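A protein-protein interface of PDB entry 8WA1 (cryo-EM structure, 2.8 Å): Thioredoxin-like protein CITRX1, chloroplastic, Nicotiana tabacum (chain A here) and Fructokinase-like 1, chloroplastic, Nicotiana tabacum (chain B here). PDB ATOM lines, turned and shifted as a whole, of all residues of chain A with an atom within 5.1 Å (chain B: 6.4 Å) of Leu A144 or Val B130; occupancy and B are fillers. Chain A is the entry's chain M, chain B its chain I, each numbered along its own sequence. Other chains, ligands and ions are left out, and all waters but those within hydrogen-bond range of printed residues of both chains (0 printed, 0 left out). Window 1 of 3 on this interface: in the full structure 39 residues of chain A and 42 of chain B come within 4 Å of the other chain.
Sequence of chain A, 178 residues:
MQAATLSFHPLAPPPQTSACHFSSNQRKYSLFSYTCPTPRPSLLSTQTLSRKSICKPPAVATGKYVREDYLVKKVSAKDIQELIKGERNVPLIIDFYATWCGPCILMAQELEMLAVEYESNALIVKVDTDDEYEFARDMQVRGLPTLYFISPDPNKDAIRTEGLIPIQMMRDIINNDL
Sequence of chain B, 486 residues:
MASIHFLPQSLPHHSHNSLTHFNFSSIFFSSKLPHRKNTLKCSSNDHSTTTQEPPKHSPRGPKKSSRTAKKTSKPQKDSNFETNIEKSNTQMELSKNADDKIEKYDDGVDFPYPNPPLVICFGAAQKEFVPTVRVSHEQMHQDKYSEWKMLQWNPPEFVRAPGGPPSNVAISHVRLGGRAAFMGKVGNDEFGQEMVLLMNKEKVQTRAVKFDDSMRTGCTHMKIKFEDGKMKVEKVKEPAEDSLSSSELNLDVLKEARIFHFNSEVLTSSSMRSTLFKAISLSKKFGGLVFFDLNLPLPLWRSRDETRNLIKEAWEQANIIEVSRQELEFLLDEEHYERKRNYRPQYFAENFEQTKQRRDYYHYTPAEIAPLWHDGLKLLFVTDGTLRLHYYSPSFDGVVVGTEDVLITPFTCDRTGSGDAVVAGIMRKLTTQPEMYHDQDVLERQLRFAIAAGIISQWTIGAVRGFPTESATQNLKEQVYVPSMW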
ATOM      1  N   PHE A  96      14.983 -20.112 -14.335  1.00  0.00           N
ATOM      2  CA  PHE A  96      14.862 -18.777 -13.776  1.00  0.00           C
ATOM      3  C   PHE A  96      13.404 -18.405 -13.881  1.00  0.00           C
ATOM      4  O   PHE A  96      12.819 -18.492 -14.954  1.00  0.00           O
ATOM      5  CB  PHE A  96      15.742 -17.795 -14.541  1.00  0.00           C
ATOM      6  CG  PHE A  96      17.212 -18.051 -14.374  1.00  0.00           C
ATOM      7  CD1 PHE A  96      17.904 -17.496 -13.312  1.00  0.00           C
ATOM      8  CD2 PHE A  96      17.901 -18.852 -15.270  1.00  0.00           C
ATOM      9  CE1 PHE A  96      19.256 -17.730 -13.149  1.00  0.00           C
ATOM     10  CE2 PHE A  96      19.250 -19.091 -15.111  1.00  0.00           C
ATOM     11  CZ  PHE A  96      19.930 -18.528 -14.050  1.00  0.00           C
ATOM     12  N   TYR A  97      12.806 -17.921 -12.816  1.00  0.00           N
ATOM     13  CA  TYR A  97      11.416 -17.613 -12.877  1.00  0.00           C
ATOM     14  C   TYR A  97      11.137 -16.383 -12.116  1.00  0.00           C
ATOM     15  O   TYR A  97      12.001 -15.890 -11.430  1.00  0.00           O
ATOM     16  CB  TYR A  97      10.622 -18.760 -12.279  1.00  0.00           C
ATOM     17  CG  TYR A  97      10.636 -18.867 -10.778  1.00  0.00           C
ATOM     18  CD1 TYR A  97      11.712 -19.413 -10.114  1.00  0.00           C
ATOM     19  CD2 TYR A  97       9.550 -18.457 -10.030  1.00  0.00           C
ATOM     20  CE1 TYR A  97      11.720 -19.518  -8.744  1.00  0.00           C
ATOM     21  CE2 TYR A  97       9.551 -18.558  -8.659  1.00  0.00           C
ATOM     22  CZ  TYR A  97      10.640 -19.092  -8.025  1.00  0.00           C
ATOM     23  OH  TYR A  97      10.644 -19.197  -6.660  1.00  0.00           O
ATOM     24  N   ALA A  98       9.949 -15.835 -12.263  1.00  0.00           N
ATOM     25  CA  ALA A  98       9.556 -14.726 -11.445  1.00  0.00           C
ATOM     26  C   ALA A  98       8.101 -14.917 -11.234  1.00  0.00           C
ATOM     27  O   ALA A  98       7.407 -15.415 -12.085  1.00  0.00           O
ATOM     28  CB  ALA A  98       9.804 -13.449 -12.139  1.00  0.00           C
ATOM     29  N   TRP A 100       5.846 -12.762 -11.117  1.00  0.00           N
ATOM     30  CA  TRP A 100       5.121 -11.919 -12.044  1.00  0.00           C
ATOM     31  C   TRP A 100       4.925 -12.410 -13.476  1.00  0.00           C
ATOM     32  O   TRP A 100       3.907 -12.107 -14.063  1.00  0.00           O
ATOM     33  CB  TRP A 100       5.657 -10.500 -12.007  1.00  0.00           C
ATOM     34  CG  TRP A 100       7.085 -10.340 -12.232  1.00  0.00           C
ATOM     35  CD1 TRP A 100       8.055 -10.270 -11.290  1.00  0.00           C
ATOM     36  CD2 TRP A 100       7.726 -10.175 -13.488  1.00  0.00           C
ATOM     37  NE1 TRP A 100       9.273 -10.091 -11.884  1.00  0.00           N
ATOM     38  CE2 TRP A 100       9.094 -10.031 -13.239  1.00  0.00           C
ATOM     39  CE3 TRP A 100       7.274 -10.146 -14.805  1.00  0.00           C
ATOM     40  CZ2 TRP A 100      10.011  -9.861 -14.252  1.00  0.00           C
ATOM     41  CZ3 TRP A 100       8.184  -9.982 -15.805  1.00  0.00           C
ATOM     42  CH2 TRP A 100       9.535  -9.843 -15.529  1.00  0.00           C
ATOM     43  N   CYS A 101       5.882 -13.100 -14.079  1.00  0.00           N
ATOM     44  CA  CYS A 101       5.709 -13.483 -15.476  1.00  0.00           C
ATOM     45  C   CYS A 101       4.619 -14.487 -15.654  1.00  0.00           C
ATOM     46  O   CYS A 101       4.577 -15.489 -14.971  1.00  0.00           O
ATOM     47  CB  CYS A 101       6.986 -14.050 -16.084  1.00  0.00           C
ATOM     48  SG  CYS A 101       7.852 -15.201 -15.003  1.00  0.00           S
ATOM     49  N   PRO A 103       4.045 -16.382 -18.457  1.00  0.00           N
ATOM     50  CA  PRO A 103       4.391 -17.647 -19.074  1.00  0.00           C
ATOM     51  C   PRO A 103       4.966 -18.617 -18.092  1.00  0.00           C
ATOM     52  O   PRO A 103       4.802 -19.808 -18.255  1.00  0.00           O
ATOM     53  CB  PRO A 103       5.438 -17.233 -20.063  1.00  0.00           C
ATOM     54  CG  PRO A 103       4.958 -15.922 -20.542  1.00  0.00           C
ATOM     55  CD  PRO A 103       4.437 -15.251 -19.314  1.00  0.00           C
ATOM     56  N   CYS A 104       5.621 -18.130 -17.067  1.00  0.00           N
ATOM     57  CA  CYS A 104       6.283 -18.984 -16.122  1.00  0.00           C
ATOM     58  C   CYS A 104       5.364 -19.902 -15.371  1.00  0.00           C
ATOM     59  O   CYS A 104       5.791 -20.934 -14.892  1.00  0.00           O
ATOM     60  CB  CYS A 104       7.086 -18.132 -15.171  1.00  0.00           C
ATOM     61  SG  CYS A 104       8.079 -16.918 -16.061  1.00  0.00           S
ATOM     62  N   THR A 129      14.424 -14.699 -10.075  1.00  0.00           N
ATOM     63  CA  THR A 129      15.169 -13.560 -10.604  1.00  0.00           C
ATOM     64  C   THR A 129      15.030 -12.340  -9.701  1.00  0.00           C
ATOM     65  O   THR A 129      15.932 -11.496  -9.647  1.00  0.00           O
ATOM     66  CB  THR A 129      14.693 -13.240 -12.021  1.00  0.00           C
ATOM     67  OG1 THR A 129      14.650 -14.449 -12.789  1.00  0.00           O
ATOM     68  CG2 THR A 129      15.641 -12.263 -12.697  1.00  0.00           C
ATOM     69  N   VAL A 141      20.847 -14.006 -19.275  1.00  0.00           N
ATOM     70  CA  VAL A 141      19.441 -14.387 -19.322  1.00  0.00           C
ATOM     71  C   VAL A 141      18.659 -13.197 -19.861  1.00  0.00           C
ATOM     72  O   VAL A 141      18.556 -12.158 -19.199  1.00  0.00           O
ATOM     73  CB  VAL A 141      18.927 -14.816 -17.941  1.00  0.00           C
ATOM     74  CG1 VAL A 141      17.454 -15.166 -18.010  1.00  0.00           C
ATOM     75  CG2 VAL A 141      19.730 -15.996 -17.419  1.00  0.00           C
ATOM     76  N   ARG A 142      18.106 -13.340 -21.068  1.00  0.00           N
ATOM     77  CA  ARG A 142      17.369 -12.235 -21.672  1.00  0.00           C
ATOM     78  C   ARG A 142      15.974 -12.095 -21.069  1.00  0.00           C
ATOM     79  O   ARG A 142      15.490 -10.975 -20.871  1.00  0.00           O
ATOM     80  CB  ARG A 142      17.276 -12.426 -23.185  1.00  0.00           C
ATOM     81  CG  ARG A 142      18.612 -12.535 -23.895  1.00  0.00           C
ATOM     82  CD  ARG A 142      18.445 -12.274 -25.383  1.00  0.00           C
ATOM     83  NE  ARG A 142      19.655 -12.585 -26.138  1.00  0.00           N
ATOM     84  CZ  ARG A 142      19.849 -13.724 -26.795  1.00  0.00           C
ATOM     85  NH1 ARG A 142      18.911 -14.659 -26.792  1.00  0.00           N
ATOM     86  NH2 ARG A 142      20.979 -13.925 -27.457  1.00  0.00           N
ATOM     87  N   GLY A 143      15.255 -13.194 -20.957  1.00  0.00           N
ATOM     88  CA  GLY A 143      13.884 -13.095 -20.516  1.00  0.00           C
ATOM     89  C   GLY A 143      13.492 -14.176 -19.592  1.00  0.00           C
ATOM     90  O   GLY A 143      14.268 -15.048 -19.316  1.00  0.00           O
ATOM     91  N   LEU A 144      12.302 -14.100 -19.051  1.00  0.00           N
ATOM     92  CA  LEU A 144      11.970 -15.069 -18.053  1.00  0.00           C
ATOM     93  C   LEU A 144      11.758 -16.539 -18.346  1.00  0.00           C
ATOM     94  O   LEU A 144      12.184 -17.381 -17.567  1.00  0.00           O
ATOM     95  CB  LEU A 144      11.016 -14.520 -17.027  1.00  0.00           C
ATOM     96  CG  LEU A 144      11.692 -14.439 -15.667  1.00  0.00           C
ATOM     97  CD1 LEU A 144      13.181 -14.706 -15.784  1.00  0.00           C
ATOM     98  CD2 LEU A 144      11.461 -13.063 -15.098  1.00  0.00           C
ATOM     99  N   PRO A 145      11.091 -16.881 -19.442  1.00  0.00           N
ATOM    100  CA  PRO A 145      10.984 -18.338 -19.595  1.00  0.00           C
ATOM    101  C   PRO A 145      12.297 -18.933 -20.112  1.00  0.00           C
ATOM    102  O   PRO A 145      12.302 -19.423 -21.219  1.00  0.00           O
ATOM    103  CB  PRO A 145       9.814 -18.510 -20.543  1.00  0.00           C
ATOM    104  CG  PRO A 145       9.128 -17.185 -20.590  1.00  0.00           C
ATOM    105  CD  PRO A 145      10.186 -16.163 -20.346  1.00  0.00           C
ATOM    106  N   THR A 146      13.364 -18.936 -19.326  1.00  0.00           N
ATOM    107  CA  THR A 146      14.693 -19.397 -19.704  1.00  0.00           C
ATOM    108  C   THR A 146      15.035 -20.645 -18.901  1.00  0.00           C
ATOM    109  O   THR A 146      14.783 -20.698 -17.692  1.00  0.00           O
ATOM    110  CB  THR A 146      15.740 -18.305 -19.465  1.00  0.00           C
ATOM    111  OG1 THR A 146      15.339 -17.103 -20.135  1.00  0.00           O
ATOM    112  CG2 THR A 146      17.098 -18.738 -19.996  1.00  0.00           C
ATOM    113  N   GLN B 126       9.771 -16.729 -30.961  1.00  0.00           N
ATOM    114  CA  GLN B 126       9.736 -17.377 -29.660  1.00  0.00           C
ATOM    115  C   GLN B 126       8.288 -17.587 -29.242  1.00  0.00           C
ATOM    116  O   GLN B 126       7.422 -16.755 -29.534  1.00  0.00           O
ATOM    117  CB  GLN B 126      10.482 -16.543 -28.609  1.00  0.00           C
ATOM    118  CG  GLN B 126      11.986 -16.471 -28.834  1.00  0.00           C
ATOM    119  CD  GLN B 126      12.626 -15.271 -28.162  1.00  0.00           C
ATOM    120  OE1 GLN B 126      12.042 -14.189 -28.111  1.00  0.00           O
ATOM    121  NE2 GLN B 126      13.835 -15.456 -27.646  1.00  0.00           N
ATOM    122  N   GLU B 128       6.601 -17.880 -26.069  1.00  0.00           N
ATOM    123  CA  GLU B 128       6.038 -16.986 -25.063  1.00  0.00           C
ATOM    124  C   GLU B 128       7.122 -16.191 -24.347  1.00  0.00           C
ATOM    125  O   GLU B 128       7.067 -16.023 -23.124  1.00  0.00           O
ATOM    126  CB  GLU B 128       5.207 -17.761 -24.035  1.00  0.00           C
ATOM    127  CG  GLU B 128       3.990 -18.475 -24.603  1.00  0.00           C
ATOM    128  CD  GLU B 128       2.920 -17.521 -25.107  1.00  0.00           C
ATOM    129  OE1 GLU B 128       2.906 -16.348 -24.677  1.00  0.00           O
ATOM    130  OE2 GLU B 128       2.088 -17.950 -25.935  1.00  0.00           O
ATOM    131  N   PHE B 129       8.113 -15.703 -25.085  1.00  0.00           N
ATOM    132  CA  PHE B 129       9.233 -15.012 -24.462  1.00  0.00           C
ATOM    133  C   PHE B 129       8.806 -13.652 -23.923  1.00  0.00           C
ATOM    134  O   PHE B 129       7.995 -12.948 -24.532  1.00  0.00           O
ATOM    135  CB  PHE B 129      10.367 -14.848 -25.471  1.00  0.00           C
ATOM    136  CG  PHE B 129      11.659 -14.396 -24.862  1.00  0.00           C
ATOM    137  CD1 PHE B 129      12.448 -15.282 -24.150  1.00  0.00           C
ATOM    138  CD2 PHE B 129      12.091 -13.090 -25.009  1.00  0.00           C
ATOM    139  CE1 PHE B 129      13.638 -14.872 -23.590  1.00  0.00           C
ATOM    140  CE2 PHE B 129      13.281 -12.675 -24.452  1.00  0.00           C
ATOM    141  CZ  PHE B 129      14.054 -13.567 -23.744  1.00  0.00           C
ATOM    142  N   VAL B 130       9.355 -13.287 -22.772  1.00  0.00           N
ATOM    143  CA  VAL B 130       9.128 -11.992 -22.139  1.00  0.00           C
ATOM    144  C   VAL B 130      10.486 -11.329 -21.934  1.00  0.00           C
ATOM    145  O   VAL B 130      11.209 -11.693 -20.998  1.00  0.00           O
ATOM    146  CB  VAL B 130       8.377 -12.131 -20.806  1.00  0.00           C
ATOM    147  CG1 VAL B 130       8.127 -10.762 -20.194  1.00  0.00           C
ATOM    148  CG2 VAL B 130       7.064 -12.876 -21.009  1.00  0.00           C
ATOM    149  N   PRO B 131      10.873 -10.364 -22.771  1.00  0.00           N
ATOM    150  CA  PRO B 131      12.210  -9.765 -22.618  1.00  0.00           C
ATOM    151  C   PRO B 131      12.305  -8.781 -21.465  1.00  0.00           C
ATOM    152  O   PRO B 131      13.359  -8.685 -20.825  1.00  0.00           O
ATOM    153  CB  PRO B 131      12.443  -9.073 -23.971  1.00  0.00           C
ATOM    154  CG  PRO B 131      11.336  -9.558 -24.880  1.00  0.00           C
ATOM    155  CD  PRO B 131      10.193  -9.885 -23.982  1.00  0.00           C
ATOM    156  N   THR B 132      11.233  -8.045 -21.182  1.00  0.00           N
ATOM    157  CA  THR B 132      11.253  -6.963 -20.199  1.00  0.00           C
ATOM    158  C   THR B 132      11.206  -7.573 -18.801  1.00  0.00           C
ATOM    159  O   THR B 132      10.139  -7.941 -18.306  1.00  0.00           O
ATOM    160  CB  THR B 132      10.087  -6.007 -20.425  1.00  0.00           C
ATOM    161  OG1 THR B 132      10.081  -5.580 -21.792  1.00  0.00           O
ATOM    162  CG2 THR B 132      10.213  -4.790 -19.523  1.00  0.00           C
ATOM    163  N   VAL B 133      12.372  -7.680 -18.169  1.00  0.00           N
ATOM    164  CA  VAL B 133      12.498  -8.235 -16.826  1.00  0.00           C
ATOM    165  C   VAL B 133      13.209  -7.217 -15.946  1.00  0.00           C
ATOM    166  O   VAL B 133      14.289  -6.727 -16.297  1.00  0.00           O
ATOM    167  CB  VAL B 133      13.256  -9.572 -16.841  1.00  0.00           C
ATOM    168  CG1 VAL B 133      13.479 -10.064 -15.423  1.00  0.00           C
ATOM    169  CG2 VAL B 133      12.495 -10.605 -17.657  1.00  0.00           C
ATOM    170  N   ARG B 134      12.607  -6.901 -14.801  1.00  0.00           N
ATOM    171  CA  ARG B 134      13.201  -6.027 -13.798  1.00  0.00           C
ATOM    172  C   ARG B 134      12.983  -6.640 -12.419  1.00  0.00           C
ATOM    173  O   ARG B 134      12.571  -7.797 -12.287  1.00  0.00           O
ATOM    174  CB  ARG B 134      12.617  -4.609 -13.869  1.00  0.00           C
ATOM    175  CG  ARG B 134      12.884  -3.890 -15.183  1.00  0.00           C
ATOM    176  CD  ARG B 134      12.520  -2.416 -15.101  1.00  0.00           C
ATOM    177  NE  ARG B 134      13.467  -1.663 -14.284  1.00  0.00           N
ATOM    178  CZ  ARG B 134      13.400  -0.351 -14.080  1.00  0.00           C
ATOM    179  NH1 ARG B 134      14.306   0.252 -13.323  1.00  0.00           N
ATOM    180  NH2 ARG B 134      12.427   0.359 -14.636  1.00  0.00           N
ATOM    181  N   PRO B 162       3.351  -5.848 -21.070  1.00  0.00           N
ATOM    182  CA  PRO B 162       4.592  -6.337 -21.679  1.00  0.00           C
ATOM    183  C   PRO B 162       4.407  -6.680 -23.149  1.00  0.00           C
ATOM    184  O   PRO B 162       3.311  -7.011 -23.605  1.00  0.00           O
ATOM    185  CB  PRO B 162       4.925  -7.590 -20.857  1.00  0.00           C
ATOM    186  CG  PRO B 162       4.082  -7.493 -19.620  1.00  0.00           C
ATOM    187  CD  PRO B 162       2.848  -6.765 -20.037  1.00  0.00           C
ATOM    188  N   GLY B 163       5.510  -6.592 -23.894  1.00  0.00           N
ATOM    189  CA  GLY B 163       5.536  -7.036 -25.266  1.00  0.00           C
ATOM    190  C   GLY B 163       6.521  -8.179 -25.415  1.00  0.00           C
ATOM    191  O   GLY B 163       7.460  -8.325 -24.634  1.00  0.00           O
ATOM    192  N   GLY B 164       6.287  -9.000 -26.435  1.00  0.00           N
ATOM    193  CA  GLY B 164       7.072 -10.195 -26.618  1.00  0.00           C
ATOM    194  C   GLY B 164       7.783 -10.261 -27.953  1.00  0.00           C
ATOM    195  O   GLY B 164       8.309  -9.265 -28.459  1.00  0.00           O
ATOM    196  N   PRO B 165       7.811 -11.450 -28.549  1.00  0.00           N
ATOM    197  CA  PRO B 165       8.555 -11.645 -29.798  1.00  0.00           C
ATOM    198  C   PRO B 165       7.903 -10.904 -30.949  1.00  0.00           C
ATOM    199  O   PRO B 165       6.703 -10.591 -30.901  1.00  0.00           O
ATOM    200  CB  PRO B 165       8.495 -13.167 -30.011  1.00  0.00           C
ATOM    201  CG  PRO B 165       8.151 -13.734 -28.666  1.00  0.00           C
ATOM    202  CD  PRO B 165       7.271 -12.713 -28.024  1.00  0.00           C
ATOM    203  N   LEU B 298      16.638  -7.941 -20.554  1.00  0.00           N
ATOM    204  CA  LEU B 298      17.223  -7.834 -19.220  1.00  0.00           C
ATOM    205  C   LEU B 298      18.581  -7.134 -19.201  1.00  0.00           C
ATOM    206  O   LEU B 298      18.767  -6.248 -18.349  1.00  0.00           O
ATOM    207  CB  LEU B 298      17.307  -9.232 -18.590  1.00  0.00           C
ATOM    208  CG  LEU B 298      17.368  -9.363 -17.066  1.00  0.00           C
ATOM    209  CD1 LEU B 298      16.922 -10.753 -16.653  1.00  0.00           C
ATOM    210  CD2 LEU B 298      18.759  -9.081 -16.522  1.00  0.00           C
ATOM    211  N   THR B 416       0.328 -10.924 -21.102  1.00  0.00           N
ATOM    212  CA  THR B 416       1.453 -11.270 -21.970  1.00  0.00           C
ATOM    213  C   THR B 416       1.433 -10.684 -23.389  1.00  0.00           C
ATOM    214  O   THR B 416       2.485 -10.299 -23.899  1.00  0.00           O
ATOM    215  CB  THR B 416       1.665 -12.797 -22.038  1.00  0.00           C
ATOM    216  OG1 THR B 416       2.736 -13.097 -22.942  1.00  0.00           O
ATOM    217  CG2 THR B 416       0.402 -13.501 -22.506  1.00  0.00           C
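O of Gly A143 is in hydrogen-bond range of OG1 of Thr A146. N of Leu B298 sits at hydrogen-bond distance from O of Pro B131 (3.4 Å). The side-chain sulfur (SG) of Cys A104 forms a disulfide with the side-chain sulfur (SG) of Cys A101, 2.0 Å away.
Of chain B, only Val B130 and Val B133 come within 4 Å of Leu A144. Val B130 touches just these residues of chain A: Pro A103 (3.7 Å), Gly A143 (3.1 Å), Leu A144 (3.3 Å) and Pro A145 (3.9 Å). Printed residues of chain B within 4 Å of Gly A143: Phe B129 (3.1 Å) and Val B130 (3.1 Å). Of the printed residues of chain A, Phe B129 touches Arg A142 and Gly A143. Of the printed residues of chain B, Pro A103 touches Glu B128 and Val B130. Of the printed residues of chain A, Glu B128 touches Pro A103 and Pro A145. Of the printed residues of chain B, Val A141 touches Leu B298 (3.2 Å). Gly B163 touches none of the printed residues of chain A. Ala A98 touches none of the printed residues of chain B. The nearest residue of chain A that does not touch Val B130 is Arg A142 (4.3 Å).
Printed residues of chain B that touch a printed residue of chain A: Glu B128, Phe B129, Val B130, Pro B131, Thr B132, Val B133, Arg B134 and Leu B298. Hydrophobic or aromatic side chains of chain B that line the printed part of chain A: Phe B129, Val B130, Val B133 and Leu B298. Among the printed residues, 15 pairs touch across the chains.
Trp A100 touches Thr B132. Val B133 touches Trp A100 (CA to CH2, 3.6 Å). CZ2 of Trp A100 touches O of Arg B134, 3.8 Å away. Glu B128 touches Pro A103 (O to CG, 3.3 Å). Val B130 touches Pro A103. Leu B298 touches Val A141 (CB to O, 3.2 Å). CZ of Phe B129 touches CB of Arg A142, 3.5 Å away. Phe B129 touches Gly A143. Gly A143 touches Val B130 (CA to O, 3.1 Å). Val B130 touches Pro A145.
The backbone carbonyl oxygen (O) of Arg A142 is in hydrogen-bond range of the backbone NH (N) of Leu B298 (3.3 Å). O of Val B130 lies within hydrogen-bond range of N of Leu A144 (3.3 Å). The backbone carbonyl oxygen of Pro B131 lies close to the backbone carbonyl oxygen of Arg A142 (3.1 Å).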
